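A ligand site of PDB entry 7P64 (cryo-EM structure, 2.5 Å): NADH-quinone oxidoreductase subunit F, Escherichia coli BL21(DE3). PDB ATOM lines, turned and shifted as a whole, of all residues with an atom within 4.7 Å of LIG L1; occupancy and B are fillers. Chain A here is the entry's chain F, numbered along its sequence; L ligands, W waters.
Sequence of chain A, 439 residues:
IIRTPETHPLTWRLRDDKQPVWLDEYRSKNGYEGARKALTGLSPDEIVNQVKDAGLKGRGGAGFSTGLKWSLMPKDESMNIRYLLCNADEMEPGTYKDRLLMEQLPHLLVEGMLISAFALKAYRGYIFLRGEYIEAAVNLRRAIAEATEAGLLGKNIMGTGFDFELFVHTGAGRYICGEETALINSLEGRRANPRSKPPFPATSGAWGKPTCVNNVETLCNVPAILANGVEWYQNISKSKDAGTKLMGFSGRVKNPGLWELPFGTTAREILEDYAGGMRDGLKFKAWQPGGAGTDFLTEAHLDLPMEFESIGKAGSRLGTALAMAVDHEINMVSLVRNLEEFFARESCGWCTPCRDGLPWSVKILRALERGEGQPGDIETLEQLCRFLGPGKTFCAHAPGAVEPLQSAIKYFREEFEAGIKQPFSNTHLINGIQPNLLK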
ATOM      1  N   GLY A  60      23.231 -11.900   5.694  1.00  0.00           N
ATOM      2  CA  GLY A  60      23.236 -13.345   5.821  1.00  0.00           C
ATOM      3  C   GLY A  60      24.625 -13.936   5.691  1.00  0.00           C
ATOM      4  O   GLY A  60      24.979 -14.883   6.398  1.00  0.00           O
ATOM      5  N   GLY A  61      25.442 -13.375   4.805  1.00  0.00           N
ATOM      6  CA  GLY A  61      26.780 -13.879   4.613  1.00  0.00           C
ATOM      7  C   GLY A  61      27.243 -13.796   3.175  1.00  0.00           C
ATOM      8  O   GLY A  61      28.413 -14.057   2.876  1.00  0.00           O
ATOM      9  N   ALA A  62      26.337 -13.450   2.270  1.00  0.00           N
ATOM     10  CA  ALA A  62      26.677 -13.321   0.859  1.00  0.00           C
ATOM     11  C   ALA A  62      26.992 -11.892   0.451  1.00  0.00           C
ATOM     12  O   ALA A  62      27.691 -11.698  -0.560  1.00  0.00           O
ATOM     13  CB  ALA A  62      25.536 -13.850  -0.007  1.00  0.00           C
ATOM     14  N   PHE A  64      25.082  -9.518  -0.782  1.00  0.00           N
ATOM     15  CA  PHE A  64      24.324  -8.942  -1.882  1.00  0.00           C
ATOM     16  C   PHE A  64      23.599  -7.684  -1.436  1.00  0.00           C
ATOM     17  O   PHE A  64      23.149  -7.593  -0.292  1.00  0.00           O
ATOM     18  CB  PHE A  64      23.326  -9.956  -2.442  1.00  0.00           C
ATOM     19  CG  PHE A  64      22.769  -9.597  -3.782  1.00  0.00           C
ATOM     20  CD1 PHE A  64      23.510  -9.798  -4.938  1.00  0.00           C
ATOM     21  CD2 PHE A  64      21.492  -9.071  -3.895  1.00  0.00           C
ATOM     22  CE1 PHE A  64      22.994  -9.469  -6.168  1.00  0.00           C
ATOM     23  CE2 PHE A  64      20.971  -8.740  -5.138  1.00  0.00           C
ATOM     24  CZ  PHE A  64      21.723  -8.947  -6.269  1.00  0.00           C
ATOM     25  N   LYS A  69      18.405  -6.107  -4.640  1.00  0.00           N
ATOM     26  CA  LYS A  69      17.472  -7.233  -4.554  1.00  0.00           C
ATOM     27  C   LYS A  69      16.024  -6.751  -4.501  1.00  0.00           C
ATOM     28  O   LYS A  69      15.138  -7.429  -5.035  1.00  0.00           O
ATOM     29  CB  LYS A  69      17.796  -8.084  -3.328  1.00  0.00           C
ATOM     30  CG  LYS A  69      17.174  -9.457  -3.345  1.00  0.00           C
ATOM     31  CD  LYS A  69      16.990  -9.998  -1.942  1.00  0.00           C
ATOM     32  CE  LYS A  69      18.313 -10.125  -1.222  1.00  0.00           C
ATOM     33  NZ  LYS A  69      18.194 -10.995  -0.030  1.00  0.00           N
ATOM     34  N   LEU A  72      14.557  -5.636  -8.072  1.00  0.00           N
ATOM     35  CA  LEU A  72      14.312  -6.661  -9.074  1.00  0.00           C
ATOM     36  C   LEU A  72      12.897  -7.224  -8.992  1.00  0.00           C
ATOM     37  O   LEU A  72      12.579  -8.157  -9.753  1.00  0.00           O
ATOM     38  CB  LEU A  72      15.339  -7.784  -8.928  1.00  0.00           C
ATOM     39  CG  LEU A  72      16.734  -7.397  -9.395  1.00  0.00           C
ATOM     40  CD1 LEU A  72      17.781  -8.313  -8.804  1.00  0.00           C
ATOM     41  CD2 LEU A  72      16.808  -7.390 -10.914  1.00  0.00           C
ATOM     42  N   GLU A  90      19.168 -19.258  11.053  1.00  0.00           N
ATOM     43  CA  GLU A  90      20.458 -19.122  11.733  1.00  0.00           C
ATOM     44  C   GLU A  90      21.005 -20.467  12.204  1.00  0.00           C
ATOM     45  O   GLU A  90      21.368 -20.650  13.362  1.00  0.00           O
ATOM     46  CB  GLU A  90      20.366 -18.137  12.904  1.00  0.00           C
ATOM     47  CG  GLU A  90      21.639 -17.346  13.141  1.00  0.00           C
ATOM     48  CD  GLU A  90      21.744 -16.825  14.555  1.00  0.00           C
ATOM     49  OE1 GLU A  90      21.150 -17.437  15.468  1.00  0.00           O
ATOM     50  OE2 GLU A  90      22.412 -15.786  14.754  1.00  0.00           O
ATOM     51  N   MET A  91      21.054 -21.419  11.274  1.00  0.00           N
ATOM     52  CA  MET A  91      21.441 -22.781  11.618  1.00  0.00           C
ATOM     53  C   MET A  91      22.932 -23.046  11.417  1.00  0.00           C
ATOM     54  O   MET A  91      23.375 -24.169  11.658  1.00  0.00           O
ATOM     55  CB  MET A  91      20.622 -23.773  10.791  1.00  0.00           C
ATOM     56  CG  MET A  91      19.403 -24.287  11.526  1.00  0.00           C
ATOM     57  SD  MET A  91      19.677 -25.895  12.280  1.00  0.00           S
ATOM     58  CE  MET A  91      18.043 -26.252  12.900  1.00  0.00           C
ATOM     59  N   GLU A  92      23.682 -22.046  10.981  1.00  0.00           N
ATOM     60  CA  GLU A  92      25.123 -22.218  10.795  1.00  0.00           C
ATOM     61  C   GLU A  92      25.816 -22.351  12.145  1.00  0.00           C
ATOM     62  O   GLU A  92      25.529 -21.566  13.055  1.00  0.00           O
ATOM     63  CB  GLU A  92      25.710 -21.050  10.025  1.00  0.00           C
ATOM     64  CG  GLU A  92      27.204 -21.136   9.784  1.00  0.00           C
ATOM     65  CD  GLU A  92      27.533 -21.764   8.450  1.00  0.00           C
ATOM     66  OE1 GLU A  92      27.259 -22.968   8.271  1.00  0.00           O
ATOM     67  OE2 GLU A  92      28.074 -21.059   7.569  1.00  0.00           O
ATOM     68  N   THR A  95      27.210 -19.277  14.717  1.00  0.00           N
ATOM     69  CA  THR A  95      26.376 -18.105  14.499  1.00  0.00           C
ATOM     70  C   THR A  95      25.334 -18.020  15.593  1.00  0.00           C
ATOM     71  O   THR A  95      24.546 -18.954  15.779  1.00  0.00           O
ATOM     72  CB  THR A  95      25.705 -18.153  13.118  1.00  0.00           C
ATOM     73  OG1 THR A  95      26.616 -18.733  12.171  1.00  0.00           O
ATOM     74  CG2 THR A  95      25.335 -16.756  12.667  1.00  0.00           C
ATOM     75  N   TYR A 175      19.194 -27.825   8.645  1.00  0.00           N
ATOM     76  CA  TYR A 175      20.136 -26.746   8.352  1.00  0.00           C
ATOM     77  C   TYR A 175      19.910 -26.157   6.956  1.00  0.00           C
ATOM     78  O   TYR A 175      20.083 -24.947   6.773  1.00  0.00           O
ATOM     79  CB  TYR A 175      21.569 -27.250   8.479  1.00  0.00           C
ATOM     80  CG  TYR A 175      22.614 -26.364   7.835  1.00  0.00           C
ATOM     81  CD1 TYR A 175      23.004 -25.177   8.444  1.00  0.00           C
ATOM     82  CD2 TYR A 175      23.224 -26.724   6.642  1.00  0.00           C
ATOM     83  CE1 TYR A 175      23.961 -24.370   7.872  1.00  0.00           C
ATOM     84  CE2 TYR A 175      24.181 -25.916   6.070  1.00  0.00           C
ATOM     85  CZ  TYR A 175      24.546 -24.753   6.683  1.00  0.00           C
ATOM     86  OH  TYR A 175      25.498 -23.950   6.104  1.00  0.00           O
ATOM     87  N   GLU A 179      18.792 -21.778   3.412  1.00  0.00           N
ATOM     88  CA  GLU A 179      18.880 -21.365   2.011  1.00  0.00           C
ATOM     89  C   GLU A 179      17.534 -20.843   1.538  1.00  0.00           C
ATOM     90  O   GLU A 179      16.489 -21.422   1.837  1.00  0.00           O
ATOM     91  CB  GLU A 179      19.315 -22.551   1.145  1.00  0.00           C
ATOM     92  CG  GLU A 179      20.104 -22.167  -0.093  1.00  0.00           C
ATOM     93  CD  GLU A 179      19.224 -22.001  -1.324  1.00  0.00           C
ATOM     94  OE1 GLU A 179      18.066 -22.440  -1.285  1.00  0.00           O
ATOM     95  OE2 GLU A 179      19.706 -21.431  -2.319  1.00  0.00           O
ATOM     96  N   GLU A 180      17.565 -19.729   0.802  1.00  0.00           N
ATOM     97  CA  GLU A 180      16.360 -18.938   0.555  1.00  0.00           C
ATOM     98  C   GLU A 180      15.305 -19.704  -0.241  1.00  0.00           C
ATOM     99  O   GLU A 180      14.111 -19.646   0.087  1.00  0.00           O
ATOM    100  CB  GLU A 180      16.717 -17.631  -0.151  1.00  0.00           C
ATOM    101  CG  GLU A 180      17.517 -17.808  -1.418  1.00  0.00           C
ATOM    102  CD  GLU A 180      17.578 -16.558  -2.261  1.00  0.00           C
ATOM    103  OE1 GLU A 180      17.012 -15.527  -1.840  1.00  0.00           O
ATOM    104  OE2 GLU A 180      18.153 -16.631  -3.357  1.00  0.00           O
ATOM    105  N   LYS A 197      18.119 -21.199  -9.800  1.00  0.00           N
ATOM    106  CA  LYS A 197      17.967 -19.806 -10.159  1.00  0.00           C
ATOM    107  C   LYS A 197      18.796 -19.513 -11.408  1.00  0.00           C
ATOM    108  O   LYS A 197      19.984 -19.874 -11.435  1.00  0.00           O
ATOM    109  CB  LYS A 197      18.406 -18.895  -9.009  1.00  0.00           C
ATOM    110  CG  LYS A 197      17.737 -19.210  -7.688  1.00  0.00           C
ATOM    111  CD  LYS A 197      18.377 -18.444  -6.538  1.00  0.00           C
ATOM    112  CE  LYS A 197      19.802 -18.905  -6.299  1.00  0.00           C
ATOM    113  NZ  LYS A 197      20.392 -18.272  -5.088  1.00  0.00           N
ATOM    114  N   PHE A 200      14.693 -16.223 -10.083  1.00  0.00           N
ATOM    115  CA  PHE A 200      14.988 -15.846  -8.719  1.00  0.00           C
ATOM    116  C   PHE A 200      13.691 -15.627  -7.946  1.00  0.00           C
ATOM    117  O   PHE A 200      12.631 -15.416  -8.542  1.00  0.00           O
ATOM    118  CB  PHE A 200      15.858 -14.594  -8.708  1.00  0.00           C
ATOM    119  CG  PHE A 200      17.280 -14.855  -9.121  1.00  0.00           C
ATOM    120  CD1 PHE A 200      18.224 -15.217  -8.172  1.00  0.00           C
ATOM    121  CD2 PHE A 200      17.656 -14.774 -10.448  1.00  0.00           C
ATOM    122  CE1 PHE A 200      19.529 -15.464  -8.552  1.00  0.00           C
ATOM    123  CE2 PHE A 200      18.962 -15.021 -10.828  1.00  0.00           C
ATOM    124  CZ  PHE A 200      19.901 -15.367  -9.874  1.00  0.00           C
ATOM    125  N   VAL A 213      13.426 -12.432   0.418  1.00  0.00           N
ATOM    126  CA  VAL A 213      13.949 -13.063   1.621  1.00  0.00           C
ATOM    127  C   VAL A 213      15.131 -12.250   2.122  1.00  0.00           C
ATOM    128  O   VAL A 213      16.070 -11.972   1.361  1.00  0.00           O
ATOM    129  CB  VAL A 213      14.372 -14.520   1.359  1.00  0.00           C
ATOM    130  CG1 VAL A 213      14.756 -15.203   2.658  1.00  0.00           C
ATOM    131  CG2 VAL A 213      13.257 -15.279   0.650  1.00  0.00           C
ATOM    132  N   ARG A 317      35.905 -16.243   3.236  1.00  0.00           N
ATOM    133  CA  ARG A 317      34.711 -15.424   3.129  1.00  0.00           C
ATOM    134  C   ARG A 317      34.446 -14.739   4.450  1.00  0.00           C
ATOM    135  O   ARG A 317      34.741 -15.284   5.520  1.00  0.00           O
ATOM    136  CB  ARG A 317      33.494 -16.260   2.737  1.00  0.00           C
ATOM    137  CG  ARG A 317      33.487 -16.778   1.317  1.00  0.00           C
ATOM    138  CD  ARG A 317      32.109 -17.283   0.941  1.00  0.00           C
ATOM    139  NE  ARG A 317      31.828 -18.608   1.475  1.00  0.00           N
ATOM    140  CZ  ARG A 317      31.139 -18.845   2.581  1.00  0.00           C
ATOM    141  NH1 ARG A 317      30.652 -17.860   3.309  1.00  0.00           N
ATOM    142  NH2 ARG A 317      30.934 -20.096   2.968  1.00  0.00           N
ATOM    143  N   GLY A 319      31.379 -14.076   5.532  1.00  0.00           N
ATOM    144  CA  GLY A 319      30.290 -14.845   6.086  1.00  0.00           C
ATOM    145  C   GLY A 319      29.429 -14.034   7.023  1.00  0.00           C
ATOM    146  O   GLY A 319      29.068 -12.879   6.749  1.00  0.00           O
ATOM    147  N   THR A 320      29.109 -14.621   8.168  1.00  0.00           N
ATOM    148  CA  THR A 320      28.321 -13.959   9.200  1.00  0.00           C
ATOM    149  C   THR A 320      29.156 -13.058  10.086  1.00  0.00           C
ATOM    150  O   THR A 320      28.608 -12.428  10.995  1.00  0.00           O
ATOM    151  CB  THR A 320      27.596 -14.994  10.067  1.00  0.00           C
ATOM    152  OG1 THR A 320      28.549 -15.684  10.882  1.00  0.00           O
ATOM    153  CG2 THR A 320      26.865 -15.991   9.190  1.00  0.00           C
ATOM    154  N   ALA A 396      24.650 -24.026  -2.788  1.00  0.00           N
ATOM    155  CA  ALA A 396      25.924 -23.577  -2.237  1.00  0.00           C
ATOM    156  C   ALA A 396      26.268 -24.235  -0.916  1.00  0.00           C
ATOM    157  O   ALA A 396      27.220 -23.803  -0.251  1.00  0.00           O
ATOM    158  CB  ALA A 396      25.912 -22.056  -2.066  1.00  0.00           C
HETATM  159  P1  LIG L   1      23.898 -16.110  -3.450  1.00  0.00           P
HETATM  160  O1  LIG L   1      25.100 -15.422  -2.936  1.00  0.00           O
HETATM  161  O2  LIG L   1      23.862 -16.300  -4.960  1.00  0.00           O
HETATM  162  O3  LIG L   1      22.564 -15.311  -3.050  1.00  0.00           O
HETATM  163  C1  LIG L   1      22.497 -14.417  -1.924  1.00  0.00           C
HETATM  164  C2  LIG L   1      21.406 -13.400  -2.160  1.00  0.00           C
HETATM  165  O4  LIG L   1      21.680 -12.674  -3.381  1.00  0.00           O
HETATM  166  C3  LIG L   1      20.003 -13.982  -2.295  1.00  0.00           C
HETATM  167  O5  LIG L   1      19.063 -13.276  -1.481  1.00  0.00           O
HETATM  168  C4  LIG L   1      19.695 -13.839  -3.792  1.00  0.00           C
HETATM  169  O6  LIG L   1      18.308 -13.595  -4.030  1.00  0.00           O
HETATM  170  C5  LIG L   1      20.515 -12.607  -4.167  1.00  0.00           C
HETATM  171  N1  LIG L   1      20.914 -12.577  -5.568  1.00  0.00           N
HETATM  172  C6  LIG L   1      22.150 -12.856  -6.090  1.00  0.00           C
HETATM  173  N2  LIG L   1      22.221 -12.743  -7.393  1.00  0.00           N
HETATM  174  C7  LIG L   1      20.935 -12.360  -7.756  1.00  0.00           C
HETATM  175  C8  LIG L   1      20.340 -12.088  -9.007  1.00  0.00           C
HETATM  176  N3  LIG L   1      21.006 -12.128 -10.169  1.00  0.00           N
HETATM  177  N4  LIG L   1      19.041 -11.751  -9.019  1.00  0.00           N
HETATM  178  C9  LIG L   1      18.375 -11.704  -7.862  1.00  0.00           C
HETATM  179  N5  LIG L   1      18.823 -11.940  -6.633  1.00  0.00           N
HETATM  180  C10 LIG L   1      20.117 -12.266  -6.639  1.00  0.00           C
HETATM  181  O7  LIG L   1      23.721 -17.551  -2.795  1.00  0.00           O
HETATM  182  P2  LIG L   1      22.951 -18.106  -1.524  1.00  0.00           P
HETATM  183  O8  LIG L   1      22.980 -19.633  -1.602  1.00  0.00           O
HETATM  184  O9  LIG L   1      21.598 -17.539  -1.398  1.00  0.00           O
HETATM  185  O10 LIG L   1      23.872 -17.702  -0.274  1.00  0.00           O
HETATM  186  C11 LIG L   1      25.185 -18.267  -0.082  1.00  0.00           C
HETATM  187  C12 LIG L   1      25.822 -17.593   1.111  1.00  0.00           C
HETATM  188  O11 LIG L   1      25.062 -17.891   2.293  1.00  0.00           O
HETATM  189  C13 LIG L   1      27.233 -18.081   1.435  1.00  0.00           C
HETATM  190  O12 LIG L   1      28.206 -17.323   0.722  1.00  0.00           O
HETATM  191  C14 LIG L   1      27.344 -17.876   2.957  1.00  0.00           C
HETATM  192  O13 LIG L   1      28.184 -16.780   3.288  1.00  0.00           O
HETATM  193  C15 LIG L   1      25.902 -17.628   3.407  1.00  0.00           C
HETATM  194  N6  LIG L   1      25.484 -18.479   4.518  1.00  0.00           N
HETATM  195  C16 LIG L   1      24.839 -17.931   5.633  1.00  0.00           C
HETATM  196  C17 LIG L   1      24.444 -18.673   6.689  1.00  0.00           C
HETATM  197  C18 LIG L   1      23.773 -17.972   7.815  1.00  0.00           C
HETATM  198  O14 LIG L   1      23.327 -16.827   7.657  1.00  0.00           O
HETATM  199  N7  LIG L   1      23.676 -18.615   8.962  1.00  0.00           N
HETATM  200  C19 LIG L   1      24.684 -20.152   6.709  1.00  0.00           C
HETATM  201  C20 LIG L   1      25.348 -20.626   5.471  1.00  0.00           C
HETATM  202  C21 LIG L   1      25.697 -19.827   4.484  1.00  0.00           C
HETATM  203  N1  LG2 L   2      20.779 -16.948   5.574  1.00  0.00           N
HETATM  204  C1  LG2 L   2      20.254 -16.638   6.810  1.00  0.00           C
HETATM  205  O1  LG2 L   2      19.909 -15.486   7.031  1.00  0.00           O
HETATM  206  N2  LG2 L   2      20.119 -17.604   7.764  1.00  0.00           N
HETATM  207  C2  LG2 L   2      20.506 -18.903   7.487  1.00  0.00           C
HETATM  208  O2  LG2 L   2      20.385 -19.767   8.341  1.00  0.00           O
HETATM  209  C3  LG2 L   2      21.041 -19.215   6.248  1.00  0.00           C
HETATM  210  N3  LG2 L   2      21.427 -20.497   5.960  1.00  0.00           N
HETATM  211  C4  LG2 L   2      21.952 -20.807   4.725  1.00  0.00           C
HETATM  212  C5  LG2 L   2      22.336 -22.114   4.471  1.00  0.00           C
HETATM  213  C6  LG2 L   2      22.876 -22.442   3.226  1.00  0.00           C
HETATM  214  C7  LG2 L   2      23.288 -23.860   2.969  1.00  0.00           C
HETATM  215  C8  LG2 L   2      23.019 -21.461   2.257  1.00  0.00           C
HETATM  216  C9  LG2 L   2      23.592 -21.803   0.919  1.00  0.00           C
HETATM  217  C10 LG2 L   2      22.626 -20.160   2.521  1.00  0.00           C
HETATM  218  C11 LG2 L   2      22.086 -19.824   3.759  1.00  0.00           C
HETATM  219  N4  LG2 L   2      21.690 -18.523   4.040  1.00  0.00           N
HETATM  220  C12 LG2 L   2      21.174 -18.232   5.282  1.00  0.00           C
HETATM  221  C13 LG2 L   2      21.820 -17.416   3.024  1.00  0.00           C
HETATM  222  C14 LG2 L   2      20.512 -17.286   2.237  1.00  0.00           C
HETATM  223  O3  LG2 L   2      20.611 -18.051   1.064  1.00  0.00           O
HETATM  224  C15 LG2 L   2      20.192 -15.838   1.870  1.00  0.00           C
HETATM  225  O4  LG2 L   2      21.339 -15.206   1.342  1.00  0.00           O
HETATM  226  C16 LG2 L   2      19.686 -15.066   3.079  1.00  0.00           C
HETATM  227  O5  LG2 L   2      18.725 -15.831   3.747  1.00  0.00           O
HETATM  228  C17 LG2 L   2      19.080 -13.716   2.725  1.00  0.00           C
HETATM  229  O6  LG2 L   2      20.030 -12.933   2.050  1.00  0.00           O
HETATM  230  P1  LG2 L   2      20.470 -11.500   2.637  1.00  0.00           P
HETATM  231  O7  LG2 L   2      21.769 -11.679   3.355  1.00  0.00           O
HETATM  232  O8  LG2 L   2      20.621 -10.512   1.504  1.00  0.00           O
HETATM  233  O9  LG2 L   2      19.442 -10.993   3.614  1.00  0.00           O
HETATM  234  O   HOH W   1      15.745 -12.581  -5.103  1.00  0.00           O
HETATM  235  O   HOH W   2      22.645 -21.919  -3.020  1.00  0.00           O
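An oxygen (O13) of LIG L1 sits at hydrogen-bond distance from the backbone carbonyl oxygen of Gly 61 (2.8 Å). An oxygen (O3) of LG2 L2 sits at hydrogen-bond distance from the backbone NH (N) of Glu 180 (3.5 Å). The side-chain amino group (NZ) of Lys 197 lies within salt-bridge range of an oxygen (O9) of LIG L1. NH1 of Arg 317 sits at hydrogen-bond distance from O13 of LIG L1 (2.7 Å). N of Met 91 is in hydrogen-bond range of O2 of LG2 L2 (3.4 Å). The backbone NH (N) of Glu 90 lies within hydrogen-bond range of an oxygen (O2) of LG2 L2 (3.0 Å). The side-chain carboxylate (OE1) of Glu 180 is in hydrogen-bond range of an oxygen (O5) of LIG L1, 3.1 Å away. O5 of LIG L1 is in hydrogen-bond range of NZ of Lys 69. An oxygen (O8) of LG2 L2 lies within salt-bridge range of the side-chain amino group (NZ) of Lys 69 (2.9 Å). N of Gly 60 is in hydrogen-bond range of O7 of LG2 L2 (2.8 Å).
An oxygen (O9) of LIG L1 is in hydrogen-bond range of an oxygen (O3) of LG2 L2 (2.7 Å).
OH of Tyr 175 lies within hydrogen-bond range of OE1 of Glu 92 (3.0 Å). The side-chain carboxylate (OE2) of Glu 180 is in salt-bridge range of the side-chain amino group (NZ) of Lys 197 (3.3 Å). The side-chain amino group (NZ) of Lys 69 sits at hydrogen-bond distance from the backbone carbonyl oxygen (O) of Val 213, at 2.7 Å. OG1 of Thr 95 sits at hydrogen-bond distance from O of Glu 92, 3.2 Å away.
An oxygen (O14) of LIG L1 lies close to the backbone carbonyl oxygen (O) of Gly 60 (2.8 Å). Residues that only touch LIG L1: Ala 62, Phe 64, Leu 72, Glu 92, Tyr 175, Glu 179, Phe 200, Thr 320 and Ala 396. Hydrophobic or aromatic side chains that line LIG L1: Ala 62, Phe 64, Leu 72, Phe 200 and Ala 396. 15 residues have an atom within 4 Å of LIG L1: Gly 60, Gly 61, Ala 62, Phe 64, Lys 69, Leu 72, Glu 92, Tyr 175, Glu 179, Glu 180, Lys 197, Phe 200, Arg 317, Thr 320 and Ala 396.
Water W2 lies within hydrogen-bond range of O8 of LIG L1 (2.7 Å), N of Ala 396 (2.9 Å) and OE2 of Glu 179 (3.1 Å).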
